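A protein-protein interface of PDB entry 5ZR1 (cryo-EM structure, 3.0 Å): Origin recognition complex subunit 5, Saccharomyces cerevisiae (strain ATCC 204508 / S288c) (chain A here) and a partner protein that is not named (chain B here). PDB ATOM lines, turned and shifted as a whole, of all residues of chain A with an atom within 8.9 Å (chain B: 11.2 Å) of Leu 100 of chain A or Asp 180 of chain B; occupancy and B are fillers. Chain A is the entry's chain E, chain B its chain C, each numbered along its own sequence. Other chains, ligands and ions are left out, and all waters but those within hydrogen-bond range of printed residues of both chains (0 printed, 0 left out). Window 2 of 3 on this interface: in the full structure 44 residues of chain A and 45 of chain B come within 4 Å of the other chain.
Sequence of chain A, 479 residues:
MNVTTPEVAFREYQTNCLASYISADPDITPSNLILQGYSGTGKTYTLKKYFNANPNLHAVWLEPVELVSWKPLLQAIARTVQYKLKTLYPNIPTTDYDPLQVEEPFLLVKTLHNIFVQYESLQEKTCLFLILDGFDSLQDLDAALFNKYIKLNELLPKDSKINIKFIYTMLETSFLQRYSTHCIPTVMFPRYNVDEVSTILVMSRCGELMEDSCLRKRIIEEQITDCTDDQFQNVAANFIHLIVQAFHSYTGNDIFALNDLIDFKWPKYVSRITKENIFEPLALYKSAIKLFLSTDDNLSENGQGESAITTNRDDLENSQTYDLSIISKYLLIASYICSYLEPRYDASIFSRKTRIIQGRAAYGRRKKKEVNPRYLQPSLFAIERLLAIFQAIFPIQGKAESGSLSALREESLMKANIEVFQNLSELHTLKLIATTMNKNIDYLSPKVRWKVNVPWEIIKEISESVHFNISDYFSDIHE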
ATOM      1  N   LYS A  71     -23.233 -22.417  20.445  1.00  0.00           N
ATOM      2  CA  LYS A  71     -23.618 -21.121  19.899  1.00  0.00           C
ATOM      3  C   LYS A  71     -23.456 -19.961  20.890  1.00  0.00           C
ATOM      4  O   LYS A  71     -23.030 -18.885  20.456  1.00  0.00           O
ATOM      5  CB  LYS A  71     -25.044 -21.203  19.348  1.00  0.00           C
ATOM      6  CG  LYS A  71     -25.541 -19.971  18.635  1.00  0.00           C
ATOM      7  CD  LYS A  71     -26.913 -20.239  18.063  1.00  0.00           C
ATOM      8  CE  LYS A  71     -27.486 -19.024  17.382  1.00  0.00           C
ATOM      9  NZ  LYS A  71     -28.831 -19.316  16.828  1.00  0.00           N
ATOM     10  N   PRO A  72     -23.750 -20.088  22.199  1.00  0.00           N
ATOM     11  CA  PRO A  72     -23.300 -19.035  23.120  1.00  0.00           C
ATOM     12  C   PRO A  72     -21.795 -18.966  23.294  1.00  0.00           C
ATOM     13  O   PRO A  72     -21.291 -17.916  23.705  1.00  0.00           O
ATOM     14  CB  PRO A  72     -23.988 -19.399  24.437  1.00  0.00           C
ATOM     15  CG  PRO A  72     -25.154 -20.137  24.047  1.00  0.00           C
ATOM     16  CD  PRO A  72     -24.740 -20.945  22.884  1.00  0.00           C
ATOM     17  N   LEU A  74     -19.595 -19.217  20.776  1.00  0.00           N
ATOM     18  CA  LEU A  74     -19.131 -18.372  19.680  1.00  0.00           C
ATOM     19  C   LEU A  74     -19.477 -16.911  19.926  1.00  0.00           C
ATOM     20  O   LEU A  74     -18.686 -16.017  19.609  1.00  0.00           O
ATOM     21  CB  LEU A  74     -19.750 -18.828  18.362  1.00  0.00           C
ATOM     22  CG  LEU A  74     -19.445 -20.211  17.798  1.00  0.00           C
ATOM     23  CD1 LEU A  74     -20.359 -20.465  16.628  1.00  0.00           C
ATOM     24  CD2 LEU A  74     -18.004 -20.332  17.371  1.00  0.00           C
ATOM     25  N   GLN A  75     -20.665 -16.654  20.475  1.00  0.00           N
ATOM     26  CA  GLN A  75     -21.122 -15.289  20.707  1.00  0.00           C
ATOM     27  C   GLN A  75     -20.335 -14.601  21.812  1.00  0.00           C
ATOM     28  O   GLN A  75     -20.127 -13.386  21.754  1.00  0.00           O
ATOM     29  CB  GLN A  75     -22.611 -15.297  21.045  1.00  0.00           C
ATOM     30  CG  GLN A  75     -23.501 -15.638  19.877  1.00  0.00           C
ATOM     31  CD  GLN A  75     -24.944 -15.793  20.274  1.00  0.00           C
ATOM     32  OE1 GLN A  75     -25.275 -15.783  21.455  1.00  0.00           O
ATOM     33  NE2 GLN A  75     -25.816 -15.926  19.287  1.00  0.00           N
ATOM     34  N   ALA A  76     -19.891 -15.353  22.818  1.00  0.00           N
ATOM     35  CA  ALA A  76     -19.095 -14.764  23.887  1.00  0.00           C
ATOM     36  C   ALA A  76     -17.673 -14.475  23.441  1.00  0.00           C
ATOM     37  O   ALA A  76     -17.032 -13.572  23.987  1.00  0.00           O
ATOM     38  CB  ALA A  76     -19.085 -15.683  25.103  1.00  0.00           C
ATOM     39  N   ALA A  78     -17.012 -13.400  20.340  1.00  0.00           N
ATOM     40  CA  ALA A  78     -17.147 -12.158  19.587  1.00  0.00           C
ATOM     41  C   ALA A  78     -17.431 -10.968  20.494  1.00  0.00           C
ATOM     42  O   ALA A  78     -17.059  -9.840  20.160  1.00  0.00           O
ATOM     43  CB  ALA A  78     -18.247 -12.299  18.540  1.00  0.00           C
ATOM     44  N   ARG A  79     -18.072 -11.194  21.641  1.00  0.00           N
ATOM     45  CA  ARG A  79     -18.357 -10.099  22.563  1.00  0.00           C
ATOM     46  C   ARG A  79     -17.111  -9.666  23.314  1.00  0.00           C
ATOM     47  O   ARG A  79     -16.803  -8.471  23.388  1.00  0.00           O
ATOM     48  CB  ARG A  79     -19.437 -10.515  23.552  1.00  0.00           C
ATOM     49  CG  ARG A  79     -19.798  -9.435  24.539  1.00  0.00           C
ATOM     50  CD  ARG A  79     -20.875  -9.906  25.485  1.00  0.00           C
ATOM     51  NE  ARG A  79     -20.416 -11.009  26.318  1.00  0.00           N
ATOM     52  CZ  ARG A  79     -20.918 -12.238  26.267  1.00  0.00           C
ATOM     53  NH1 ARG A  79     -21.897 -12.517  25.420  1.00  0.00           N
ATOM     54  NH2 ARG A  79     -20.440 -13.183  27.063  1.00  0.00           N
ATOM     55  N   GLN A  82     -13.906  -7.922  21.255  1.00  0.00           N
ATOM     56  CA  GLN A  82     -14.022  -6.510  20.917  1.00  0.00           C
ATOM     57  C   GLN A  82     -14.167  -5.641  22.158  1.00  0.00           C
ATOM     58  O   GLN A  82     -13.769  -4.474  22.134  1.00  0.00           O
ATOM     59  CB  GLN A  82     -15.179  -6.280  19.946  1.00  0.00           C
ATOM     60  CG  GLN A  82     -16.552  -6.607  20.474  1.00  0.00           C
ATOM     61  CD  GLN A  82     -17.627  -6.369  19.436  1.00  0.00           C
ATOM     62  OE1 GLN A  82     -17.350  -5.877  18.344  1.00  0.00           O
ATOM     63  NE2 GLN A  82     -18.860  -6.718  19.771  1.00  0.00           N
ATOM     64  N   TYR A  97     -19.650  -4.351  16.263  1.00  0.00           N
ATOM     65  CA  TYR A  97     -20.405  -5.416  15.625  1.00  0.00           C
ATOM     66  C   TYR A  97     -21.182  -6.160  16.696  1.00  0.00           C
ATOM     67  O   TYR A  97     -20.667  -6.404  17.789  1.00  0.00           O
ATOM     68  CB  TYR A  97     -19.470  -6.371  14.884  1.00  0.00           C
ATOM     69  CG  TYR A  97     -18.733  -5.721  13.742  1.00  0.00           C
ATOM     70  CD1 TYR A  97     -19.309  -5.624  12.484  1.00  0.00           C
ATOM     71  CD2 TYR A  97     -17.473  -5.173  13.930  1.00  0.00           C
ATOM     72  CE1 TYR A  97     -18.638  -5.020  11.437  1.00  0.00           C
ATOM     73  CE2 TYR A  97     -16.796  -4.566  12.895  1.00  0.00           C
ATOM     74  CZ  TYR A  97     -17.382  -4.491  11.652  1.00  0.00           C
ATOM     75  OH  TYR A  97     -16.703  -3.885  10.621  1.00  0.00           O
ATOM     76  N   ASP A  98     -22.427  -6.484  16.391  1.00  0.00           N
ATOM     77  CA  ASP A  98     -23.290  -7.171  17.340  1.00  0.00           C
ATOM     78  C   ASP A  98     -22.785  -8.596  17.537  1.00  0.00           C
ATOM     79  O   ASP A  98     -22.728  -9.358  16.564  1.00  0.00           O
ATOM     80  CB  ASP A  98     -24.726  -7.172  16.818  1.00  0.00           C
ATOM     81  CG  ASP A  98     -25.752  -7.534  17.882  1.00  0.00           C
ATOM     82  OD1 ASP A  98     -25.381  -7.754  19.050  1.00  0.00           O
ATOM     83  OD2 ASP A  98     -26.950  -7.603  17.540  1.00  0.00           O
ATOM     84  N   PRO A  99     -22.387  -8.990  18.751  1.00  0.00           N
ATOM     85  CA  PRO A  99     -21.928 -10.371  18.957  1.00  0.00           C
ATOM     86  C   PRO A  99     -23.039 -11.389  18.880  1.00  0.00           C
ATOM     87  O   PRO A  99     -22.758 -12.577  18.707  1.00  0.00           O
ATOM     88  CB  PRO A  99     -21.324 -10.330  20.360  1.00  0.00           C
ATOM     89  CG  PRO A  99     -22.049  -9.238  21.039  1.00  0.00           C
ATOM     90  CD  PRO A  99     -22.298  -8.201  19.990  1.00  0.00           C
ATOM     91  N   LEU A 100     -24.287 -10.967  18.995  1.00  0.00           N
ATOM     92  CA  LEU A 100     -25.419 -11.872  18.905  1.00  0.00           C
ATOM     93  C   LEU A 100     -25.780 -12.182  17.457  1.00  0.00           C
ATOM     94  O   LEU A 100     -26.660 -13.010  17.207  1.00  0.00           O
ATOM     95  CB  LEU A 100     -26.590 -11.250  19.665  1.00  0.00           C
ATOM     96  CG  LEU A 100     -27.811 -12.038  20.100  1.00  0.00           C
ATOM     97  CD1 LEU A 100     -27.392 -13.174  20.990  1.00  0.00           C
ATOM     98  CD2 LEU A 100     -28.671 -11.097  20.865  1.00  0.00           C
ATOM     99  N   GLN A 101     -25.085 -11.560  16.507  1.00  0.00           N
ATOM    100  CA  GLN A 101     -25.299 -11.796  15.090  1.00  0.00           C
ATOM    101  C   GLN A 101     -24.548 -13.026  14.591  1.00  0.00           C
ATOM    102  O   GLN A 101     -24.891 -13.556  13.529  1.00  0.00           O
ATOM    103  CB  GLN A 101     -24.870 -10.550  14.310  1.00  0.00           C
ATOM    104  CG  GLN A 101     -25.375 -10.447  12.886  1.00  0.00           C
ATOM    105  CD  GLN A 101     -24.945  -9.163  12.217  1.00  0.00           C
ATOM    106  OE1 GLN A 101     -24.149  -8.404  12.764  1.00  0.00           O
ATOM    107  NE2 GLN A 101     -25.495  -8.898  11.040  1.00  0.00           N
ATOM    108  N   VAL A 102     -23.549 -13.510  15.325  1.00  0.00           N
ATOM    109  CA  VAL A 102     -22.863 -14.727  14.905  1.00  0.00           C
ATOM    110  C   VAL A 102     -23.716 -15.926  15.304  1.00  0.00           C
ATOM    111  O   VAL A 102     -24.245 -16.007  16.420  1.00  0.00           O
ATOM    112  CB  VAL A 102     -21.424 -14.795  15.461  1.00  0.00           C
ATOM    113  CG1 VAL A 102     -20.671 -13.569  15.057  1.00  0.00           C
ATOM    114  CG2 VAL A 102     -21.335 -14.937  16.951  1.00  0.00           C
ATOM    115  N   GLU A 103     -23.961 -16.798  14.338  1.00  0.00           N
ATOM    116  CA  GLU A 103     -24.832 -17.947  14.529  1.00  0.00           C
ATOM    117  C   GLU A 103     -24.206 -19.177  13.896  1.00  0.00           C
ATOM    118  O   GLU A 103     -24.840 -20.238  13.864  1.00  0.00           O
ATOM    119  CB  GLU A 103     -26.220 -17.683  13.923  1.00  0.00           C
ATOM    120  CG  GLU A 103     -27.000 -16.569  14.610  1.00  0.00           C
ATOM    121  CD  GLU A 103     -28.293 -16.218  13.920  1.00  0.00           C
ATOM    122  OE1 GLU A 103     -28.565 -16.768  12.834  1.00  0.00           O
ATOM    123  OE2 GLU A 103     -29.033 -15.373  14.462  1.00  0.00           O
ATOM    124  N   GLU A 104     -22.990 -19.047  13.383  1.00  0.00           N
ATOM    125  CA  GLU A 104     -22.262 -20.039  12.620  1.00  0.00           C
ATOM    126  C   GLU A 104     -20.820 -20.007  13.094  1.00  0.00           C
ATOM    127  O   GLU A 104     -20.369 -18.989  13.631  1.00  0.00           O
ATOM    128  CB  GLU A 104     -22.296 -19.728  11.114  1.00  0.00           C
ATOM    129  CG  GLU A 104     -23.674 -19.653  10.476  1.00  0.00           C
ATOM    130  CD  GLU A 104     -24.352 -20.992  10.363  1.00  0.00           C
ATOM    131  OE1 GLU A 104     -23.644 -21.996  10.144  1.00  0.00           O
ATOM    132  OE2 GLU A 104     -25.592 -21.043  10.489  1.00  0.00           O
ATOM    133  N   LEU A 107     -19.492 -17.325  10.671  1.00  0.00           N
ATOM    134  CA  LEU A 107     -19.832 -15.950  11.009  1.00  0.00           C
ATOM    135  C   LEU A 107     -19.005 -15.419  12.167  1.00  0.00           C
ATOM    136  O   LEU A 107     -18.918 -14.202  12.333  1.00  0.00           O
ATOM    137  CB  LEU A 107     -21.310 -15.826  11.343  1.00  0.00           C
ATOM    138  CG  LEU A 107     -22.267 -16.044  10.180  1.00  0.00           C
ATOM    139  CD1 LEU A 107     -23.672 -15.987  10.686  1.00  0.00           C
ATOM    140  CD2 LEU A 107     -22.055 -15.007   9.107  1.00  0.00           C
ATOM    141  N   THR A 111     -16.787 -12.130  11.473  1.00  0.00           N
ATOM    142  CA  THR A 111     -16.826 -11.051  12.456  1.00  0.00           C
ATOM    143  C   THR A 111     -15.438 -10.741  12.997  1.00  0.00           C
ATOM    144  O   THR A 111     -15.068  -9.568  13.120  1.00  0.00           O
ATOM    145  CB  THR A 111     -17.786 -11.413  13.586  1.00  0.00           C
ATOM    146  OG1 THR A 111     -19.102 -11.552  13.043  1.00  0.00           O
ATOM    147  CG2 THR A 111     -17.811 -10.352  14.665  1.00  0.00           C
ATOM    148  N   ARG B 144     -31.686 -21.825  29.816  1.00  0.00           N
ATOM    149  CA  ARG B 144     -32.321 -20.915  28.870  1.00  0.00           C
ATOM    150  C   ARG B 144     -33.714 -20.491  29.302  1.00  0.00           C
ATOM    151  O   ARG B 144     -34.187 -19.443  28.861  1.00  0.00           O
ATOM    152  CB  ARG B 144     -32.391 -21.543  27.483  1.00  0.00           C
ATOM    153  CG  ARG B 144     -31.056 -21.698  26.817  1.00  0.00           C
ATOM    154  CD  ARG B 144     -31.214 -22.266  25.435  1.00  0.00           C
ATOM    155  NE  ARG B 144     -31.959 -21.358  24.577  1.00  0.00           N
ATOM    156  CZ  ARG B 144     -31.414 -20.359  23.896  1.00  0.00           C
ATOM    157  NH1 ARG B 144     -32.173 -19.581  23.143  1.00  0.00           N
ATOM    158  NH2 ARG B 144     -30.110 -20.138  23.968  1.00  0.00           N
ATOM    159  N   MET B 147     -32.678 -17.921  32.409  1.00  0.00           N
ATOM    160  CA  MET B 147     -32.184 -16.643  31.929  1.00  0.00           C
ATOM    161  C   MET B 147     -33.228 -15.889  31.130  1.00  0.00           C
ATOM    162  O   MET B 147     -33.127 -14.667  31.001  1.00  0.00           O
ATOM    163  CB  MET B 147     -30.935 -16.849  31.083  1.00  0.00           C
ATOM    164  CG  MET B 147     -29.776 -17.454  31.835  1.00  0.00           C
ATOM    165  SD  MET B 147     -29.223 -16.488  33.247  1.00  0.00           S
ATOM    166  CE  MET B 147     -29.718 -17.547  34.598  1.00  0.00           C
ATOM    167  N   TYR B 148     -34.224 -16.584  30.593  1.00  0.00           N
ATOM    168  CA  TYR B 148     -35.350 -15.876  30.009  1.00  0.00           C
ATOM    169  C   TYR B 148     -36.281 -15.348  31.089  1.00  0.00           C
ATOM    170  O   TYR B 148     -36.820 -14.250  30.953  1.00  0.00           O
ATOM    171  CB  TYR B 148     -36.105 -16.779  29.037  1.00  0.00           C
ATOM    172  CG  TYR B 148     -37.327 -16.126  28.445  1.00  0.00           C
ATOM    173  CD1 TYR B 148     -37.208 -15.121  27.502  1.00  0.00           C
ATOM    174  CD2 TYR B 148     -38.599 -16.525  28.823  1.00  0.00           C
ATOM    175  CE1 TYR B 148     -38.319 -14.521  26.963  1.00  0.00           C
ATOM    176  CE2 TYR B 148     -39.716 -15.935  28.284  1.00  0.00           C
ATOM    177  CZ  TYR B 148     -39.569 -14.931  27.356  1.00  0.00           C
ATOM    178  OH  TYR B 148     -40.677 -14.334  26.812  1.00  0.00           O
ATOM    179  N   TYR B 151     -34.588 -12.159  32.637  1.00  0.00           N
ATOM    180  CA  TYR B 151     -34.506 -11.029  31.725  1.00  0.00           C
ATOM    181  C   TYR B 151     -35.889 -10.501  31.377  1.00  0.00           C
ATOM    182  O   TYR B 151     -36.047  -9.302  31.128  1.00  0.00           O
ATOM    183  CB  TYR B 151     -33.755 -11.427  30.460  1.00  0.00           C
ATOM    184  CG  TYR B 151     -33.482 -10.268  29.542  1.00  0.00           C
ATOM    185  CD1 TYR B 151     -32.489  -9.349  29.841  1.00  0.00           C
ATOM    186  CD2 TYR B 151     -34.212 -10.089  28.378  1.00  0.00           C
ATOM    187  CE1 TYR B 151     -32.231  -8.288  29.011  1.00  0.00           C
ATOM    188  CE2 TYR B 151     -33.961  -9.027  27.539  1.00  0.00           C
ATOM    189  CZ  TYR B 151     -32.968  -8.131  27.861  1.00  0.00           C
ATOM    190  OH  TYR B 151     -32.709  -7.068  27.033  1.00  0.00           O
ATOM    191  N   SER B 152     -36.898 -11.371  31.359  1.00  0.00           N
ATOM    192  CA  SER B 152     -38.259 -10.903  31.128  1.00  0.00           C
ATOM    193  C   SER B 152     -38.818 -10.218  32.365  1.00  0.00           C
ATOM    194  O   SER B 152     -39.558  -9.235  32.253  1.00  0.00           O
ATOM    195  CB  SER B 152     -39.156 -12.064  30.707  1.00  0.00           C
ATOM    196  OG  SER B 152     -40.481 -11.629  30.477  1.00  0.00           O
ATOM    197  N   ASP B 155     -37.159  -6.572  32.779  1.00  0.00           N
ATOM    198  CA  ASP B 155     -37.734  -5.553  31.915  1.00  0.00           C
ATOM    199  C   ASP B 155     -39.160  -5.209  32.309  1.00  0.00           C
ATOM    200  O   ASP B 155     -39.653  -4.141  31.934  1.00  0.00           O
ATOM    201  CB  ASP B 155     -37.701  -6.010  30.459  1.00  0.00           C
ATOM    202  CG  ASP B 155     -36.303  -6.057  29.902  1.00  0.00           C
ATOM    203  OD1 ASP B 155     -35.452  -5.277  30.373  1.00  0.00           O
ATOM    204  OD2 ASP B 155     -36.052  -6.871  28.991  1.00  0.00           O
ATOM    205  N   ASN B 179     -32.741  -3.959  23.210  1.00  0.00           N
ATOM    206  CA  ASN B 179     -31.673  -4.870  22.817  1.00  0.00           C
ATOM    207  C   ASN B 179     -31.914  -6.293  23.320  1.00  0.00           C
ATOM    208  O   ASN B 179     -32.649  -6.505  24.281  1.00  0.00           O
ATOM    209  CB  ASN B 179     -30.317  -4.341  23.304  1.00  0.00           C
ATOM    210  CG  ASN B 179     -30.298  -4.023  24.792  1.00  0.00           C
ATOM    211  OD1 ASN B 179     -31.279  -4.233  25.506  1.00  0.00           O
ATOM    212  ND2 ASN B 179     -29.170  -3.511  25.267  1.00  0.00           N
ATOM    213  N   ASP B 180     -31.296  -7.261  22.654  1.00  0.00           N
ATOM    214  CA  ASP B 180     -31.474  -8.670  22.962  1.00  0.00           C
ATOM    215  C   ASP B 180     -30.216  -9.236  23.599  1.00  0.00           C
ATOM    216  O   ASP B 180     -29.106  -8.736  23.399  1.00  0.00           O
ATOM    217  CB  ASP B 180     -31.817  -9.468  21.706  1.00  0.00           C
ATOM    218  CG  ASP B 180     -33.188  -9.160  21.181  1.00  0.00           C
ATOM    219  OD1 ASP B 180     -34.090  -8.877  21.997  1.00  0.00           O
ATOM    220  OD2 ASP B 180     -33.357  -9.182  19.946  1.00  0.00           O
ATOM    221  N   VAL B 181     -30.409 -10.301  24.372  1.00  0.00           N
ATOM    222  CA  VAL B 181     -29.361 -10.912  25.180  1.00  0.00           C
ATOM    223  C   VAL B 181     -29.369 -12.413  24.919  1.00  0.00           C
ATOM    224  O   VAL B 181     -30.437 -13.029  24.834  1.00  0.00           O
ATOM    225  CB  VAL B 181     -29.572 -10.593  26.682  1.00  0.00           C
ATOM    226  CG1 VAL B 181     -28.636 -11.376  27.566  1.00  0.00           C
ATOM    227  CG2 VAL B 181     -29.361  -9.114  26.947  1.00  0.00           C
ATOM    228  N   SER B 182     -28.181 -12.989  24.737  1.00  0.00           N
ATOM    229  CA  SER B 182     -28.035 -14.439  24.729  1.00  0.00           C
ATOM    230  C   SER B 182     -28.393 -15.003  26.098  1.00  0.00           C
ATOM    231  O   SER B 182     -27.841 -14.576  27.116  1.00  0.00           O
ATOM    232  CB  SER B 182     -26.602 -14.819  24.363  1.00  0.00           C
ATOM    233  OG  SER B 182     -26.419 -16.221  24.402  1.00  0.00           O
ATOM    234  N   TYR B 183     -29.319 -15.961  26.131  1.00  0.00           N
ATOM    235  CA  TYR B 183     -29.824 -16.461  27.410  1.00  0.00           C
ATOM    236  C   TYR B 183     -28.888 -17.544  27.919  1.00  0.00           C
ATOM    237  O   TYR B 183     -29.030 -18.726  27.611  1.00  0.00           O
ATOM    238  CB  TYR B 183     -31.249 -16.979  27.284  1.00  0.00           C
ATOM    239  CG  TYR B 183     -32.203 -15.946  26.767  1.00  0.00           C
ATOM    240  CD1 TYR B 183     -32.407 -14.763  27.454  1.00  0.00           C
ATOM    241  CD2 TYR B 183     -32.954 -16.184  25.630  1.00  0.00           C
ATOM    242  CE1 TYR B 183     -33.282 -13.818  26.988  1.00  0.00           C
ATOM    243  CE2 TYR B 183     -33.841 -15.250  25.163  1.00  0.00           C
ATOM    244  CZ  TYR B 183     -34.001 -14.072  25.848  1.00  0.00           C
ATOM    245  OH  TYR B 183     -34.886 -13.134  25.386  1.00  0.00           O
ATOM    246  N   ASP B 184     -27.918 -17.119  28.718  1.00  0.00           N
ATOM    247  CA  ASP B 184     -26.974 -18.003  29.376  1.00  0.00           C
ATOM    248  C   ASP B 184     -26.476 -17.291  30.628  1.00  0.00           C
ATOM    249  O   ASP B 184     -26.907 -16.178  30.938  1.00  0.00           O
ATOM    250  CB  ASP B 184     -25.854 -18.407  28.407  1.00  0.00           C
ATOM    251  CG  ASP B 184     -25.157 -17.217  27.782  1.00  0.00           C
ATOM    252  OD1 ASP B 184     -25.539 -16.059  28.032  1.00  0.00           O
ATOM    253  OD2 ASP B 184     -24.218 -17.438  27.006  1.00  0.00           O
ATOM    254  N   SER B 186     -23.905 -15.715  31.341  1.00  0.00           N
ATOM    255  CA  SER B 186     -23.253 -14.427  31.158  1.00  0.00           C
ATOM    256  C   SER B 186     -24.215 -13.259  31.321  1.00  0.00           C
ATOM    257  O   SER B 186     -23.769 -12.110  31.346  1.00  0.00           O
ATOM    258  CB  SER B 186     -22.601 -14.364  29.778  1.00  0.00           C
ATOM    259  OG  SER B 186     -23.580 -14.402  28.758  1.00  0.00           O
ATOM    260  N   LEU B 187     -25.519 -13.519  31.412  1.00  0.00           N
ATOM    261  CA  LEU B 187     -26.466 -12.476  31.785  1.00  0.00           C
ATOM    262  C   LEU B 187     -26.357 -12.133  33.264  1.00  0.00           C
ATOM    263  O   LEU B 187     -26.679 -11.011  33.671  1.00  0.00           O
ATOM    264  CB  LEU B 187     -27.881 -12.929  31.425  1.00  0.00           C
ATOM    265  CG  LEU B 187     -29.107 -12.103  31.800  1.00  0.00           C
ATOM    266  CD1 LEU B 187     -29.011 -10.700  31.244  1.00  0.00           C
ATOM    267  CD2 LEU B 187     -30.336 -12.802  31.276  1.00  0.00           C
ATOM    268  N   ASN B 190     -23.346  -9.617  33.607  1.00  0.00           N
ATOM    269  CA  ASN B 190     -23.628  -8.315  33.027  1.00  0.00           C
ATOM    270  C   ASN B 190     -24.845  -7.654  33.644  1.00  0.00           C
ATOM    271  O   ASN B 190     -25.380  -6.713  33.057  1.00  0.00           O
ATOM    272  CB  ASN B 190     -23.824  -8.432  31.514  1.00  0.00           C
ATOM    273  CG  ASN B 190     -22.553  -8.800  30.786  1.00  0.00           C
ATOM    274  OD1 ASN B 190     -22.458  -9.856  30.167  1.00  0.00           O
ATOM    275  ND2 ASN B 190     -21.567  -7.922  30.850  1.00  0.00           N
ATOM    276  N   LEU B 194     -25.840  -3.591  33.106  1.00  0.00           N
ATOM    277  CA  LEU B 194     -26.937  -3.373  32.177  1.00  0.00           C
ATOM    278  C   LEU B 194     -28.215  -2.907  32.854  1.00  0.00           C
ATOM    279  O   LEU B 194     -29.075  -2.337  32.175  1.00  0.00           O
ATOM    280  CB  LEU B 194     -27.207  -4.665  31.389  1.00  0.00           C
ATOM    281  CG  LEU B 194     -28.005  -4.801  30.100  1.00  0.00           C
ATOM    282  CD1 LEU B 194     -27.382  -5.935  29.310  1.00  0.00           C
ATOM    283  CD2 LEU B 194     -29.458  -5.106  30.368  1.00  0.00           C
ATOM    284  N   PHE B 195     -28.357  -3.104  34.165  1.00  0.00           N
ATOM    285  CA  PHE B 195     -29.543  -2.706  34.908  1.00  0.00           C
ATOM    286  C   PHE B 195     -29.251  -1.818  36.107  1.00  0.00           C
ATOM    287  O   PHE B 195     -30.193  -1.247  36.666  1.00  0.00           O
ATOM    288  CB  PHE B 195     -30.309  -3.949  35.375  1.00  0.00           C
ATOM    289  CG  PHE B 195     -31.106  -4.604  34.291  1.00  0.00           C
ATOM    290  CD1 PHE B 195     -31.700  -3.851  33.296  1.00  0.00           C
ATOM    291  CD2 PHE B 195     -31.183  -5.977  34.212  1.00  0.00           C
ATOM    292  CE1 PHE B 195     -32.426  -4.462  32.288  1.00  0.00           C
ATOM    293  CE2 PHE B 195     -31.886  -6.594  33.200  1.00  0.00           C
ATOM    294  CZ  PHE B 195     -32.513  -5.839  32.241  1.00  0.00           C
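The side-chain amide oxygen (OD1) of Asn 190 of chain B sits close to the backbone carbonyl oxygen (O) of Ser 186 of chain B.
The side-chain carboxylate of Asp 98 of chain A lies close to the backbone NH of Leu 100 of chain A (3.4 Å).
The side-chain amide nitrogen of Gln 75 of chain A is in hydrogen-bond range of the backbone carbonyl oxygen of Val 102 of chain A, at 3.3 Å.
The side-chain hydroxyl (OG) of Ser 186 of chain B lies within hydrogen-bond range of the side-chain carboxylate (OD1) of Asp 184 of chain B, 2.7 Å away.
The side-chain hydroxyl (OG) of Ser 182 of chain B is in hydrogen-bond range of the side-chain amide oxygen (OE1) of Gln 75 of chain A (3.2 Å).
Of the 18 printed residues of chain A, 4 touch a printed residue of chain B.
Printed residues of chain A that touch a printed residue of chain B: Pro 72, Gln 75, Arg 79 and Leu 100.
Hydrophobic or aromatic side chains of chain A within 4 Å of the printed part of chain B: Pro 72 and Leu 100.
Of the 17 printed residues of chain B, 5 touch a printed residue of chain A.
Among the printed residues, 6 pairs touch across the chains.
Among the printed residues, no Asp or Glu carboxylate lies within 4 Å of a Lys or Arg side-chain nitrogen of the other chain.
Among the printed residues, pairs that only touch across the chains: Pro 72 of chain A with Asp 184 of chain B (3.2 Å), Leu 100 of chain A with Asp 180 of chain B (3.5 Å), Arg 79 of chain A with Ser 186 of chain B (3.7 Å), Leu 100 of chain A with Ser 182 of chain B (3.8 Å) and Leu 100 of chain A with Val 181 of chain B (3.99 Å).
Of the printed residues of chain B, Pro 72 of chain A touches Asp 184.
Printed residues of chain B within 4 Å of Arg 79 of chain A: Ser 186 (3.7 Å).
No residue of chain B comes within 4 Å of Asp 98 of chain A.
Val 102 of chain A touches none of the printed residues of chain B.
Of the printed residues of chain A, Asp 180 of chain B touches Leu 100.
Printed residues of chain A within 4 Å of Ser 182 of chain B: Gln 75 and Leu 100.
Of the printed residues of chain A, Asp 184 of chain B touches Pro 72.
Of the printed residues of chain A, Ser 186 of chain B touches Arg 79 (3.7 Å).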
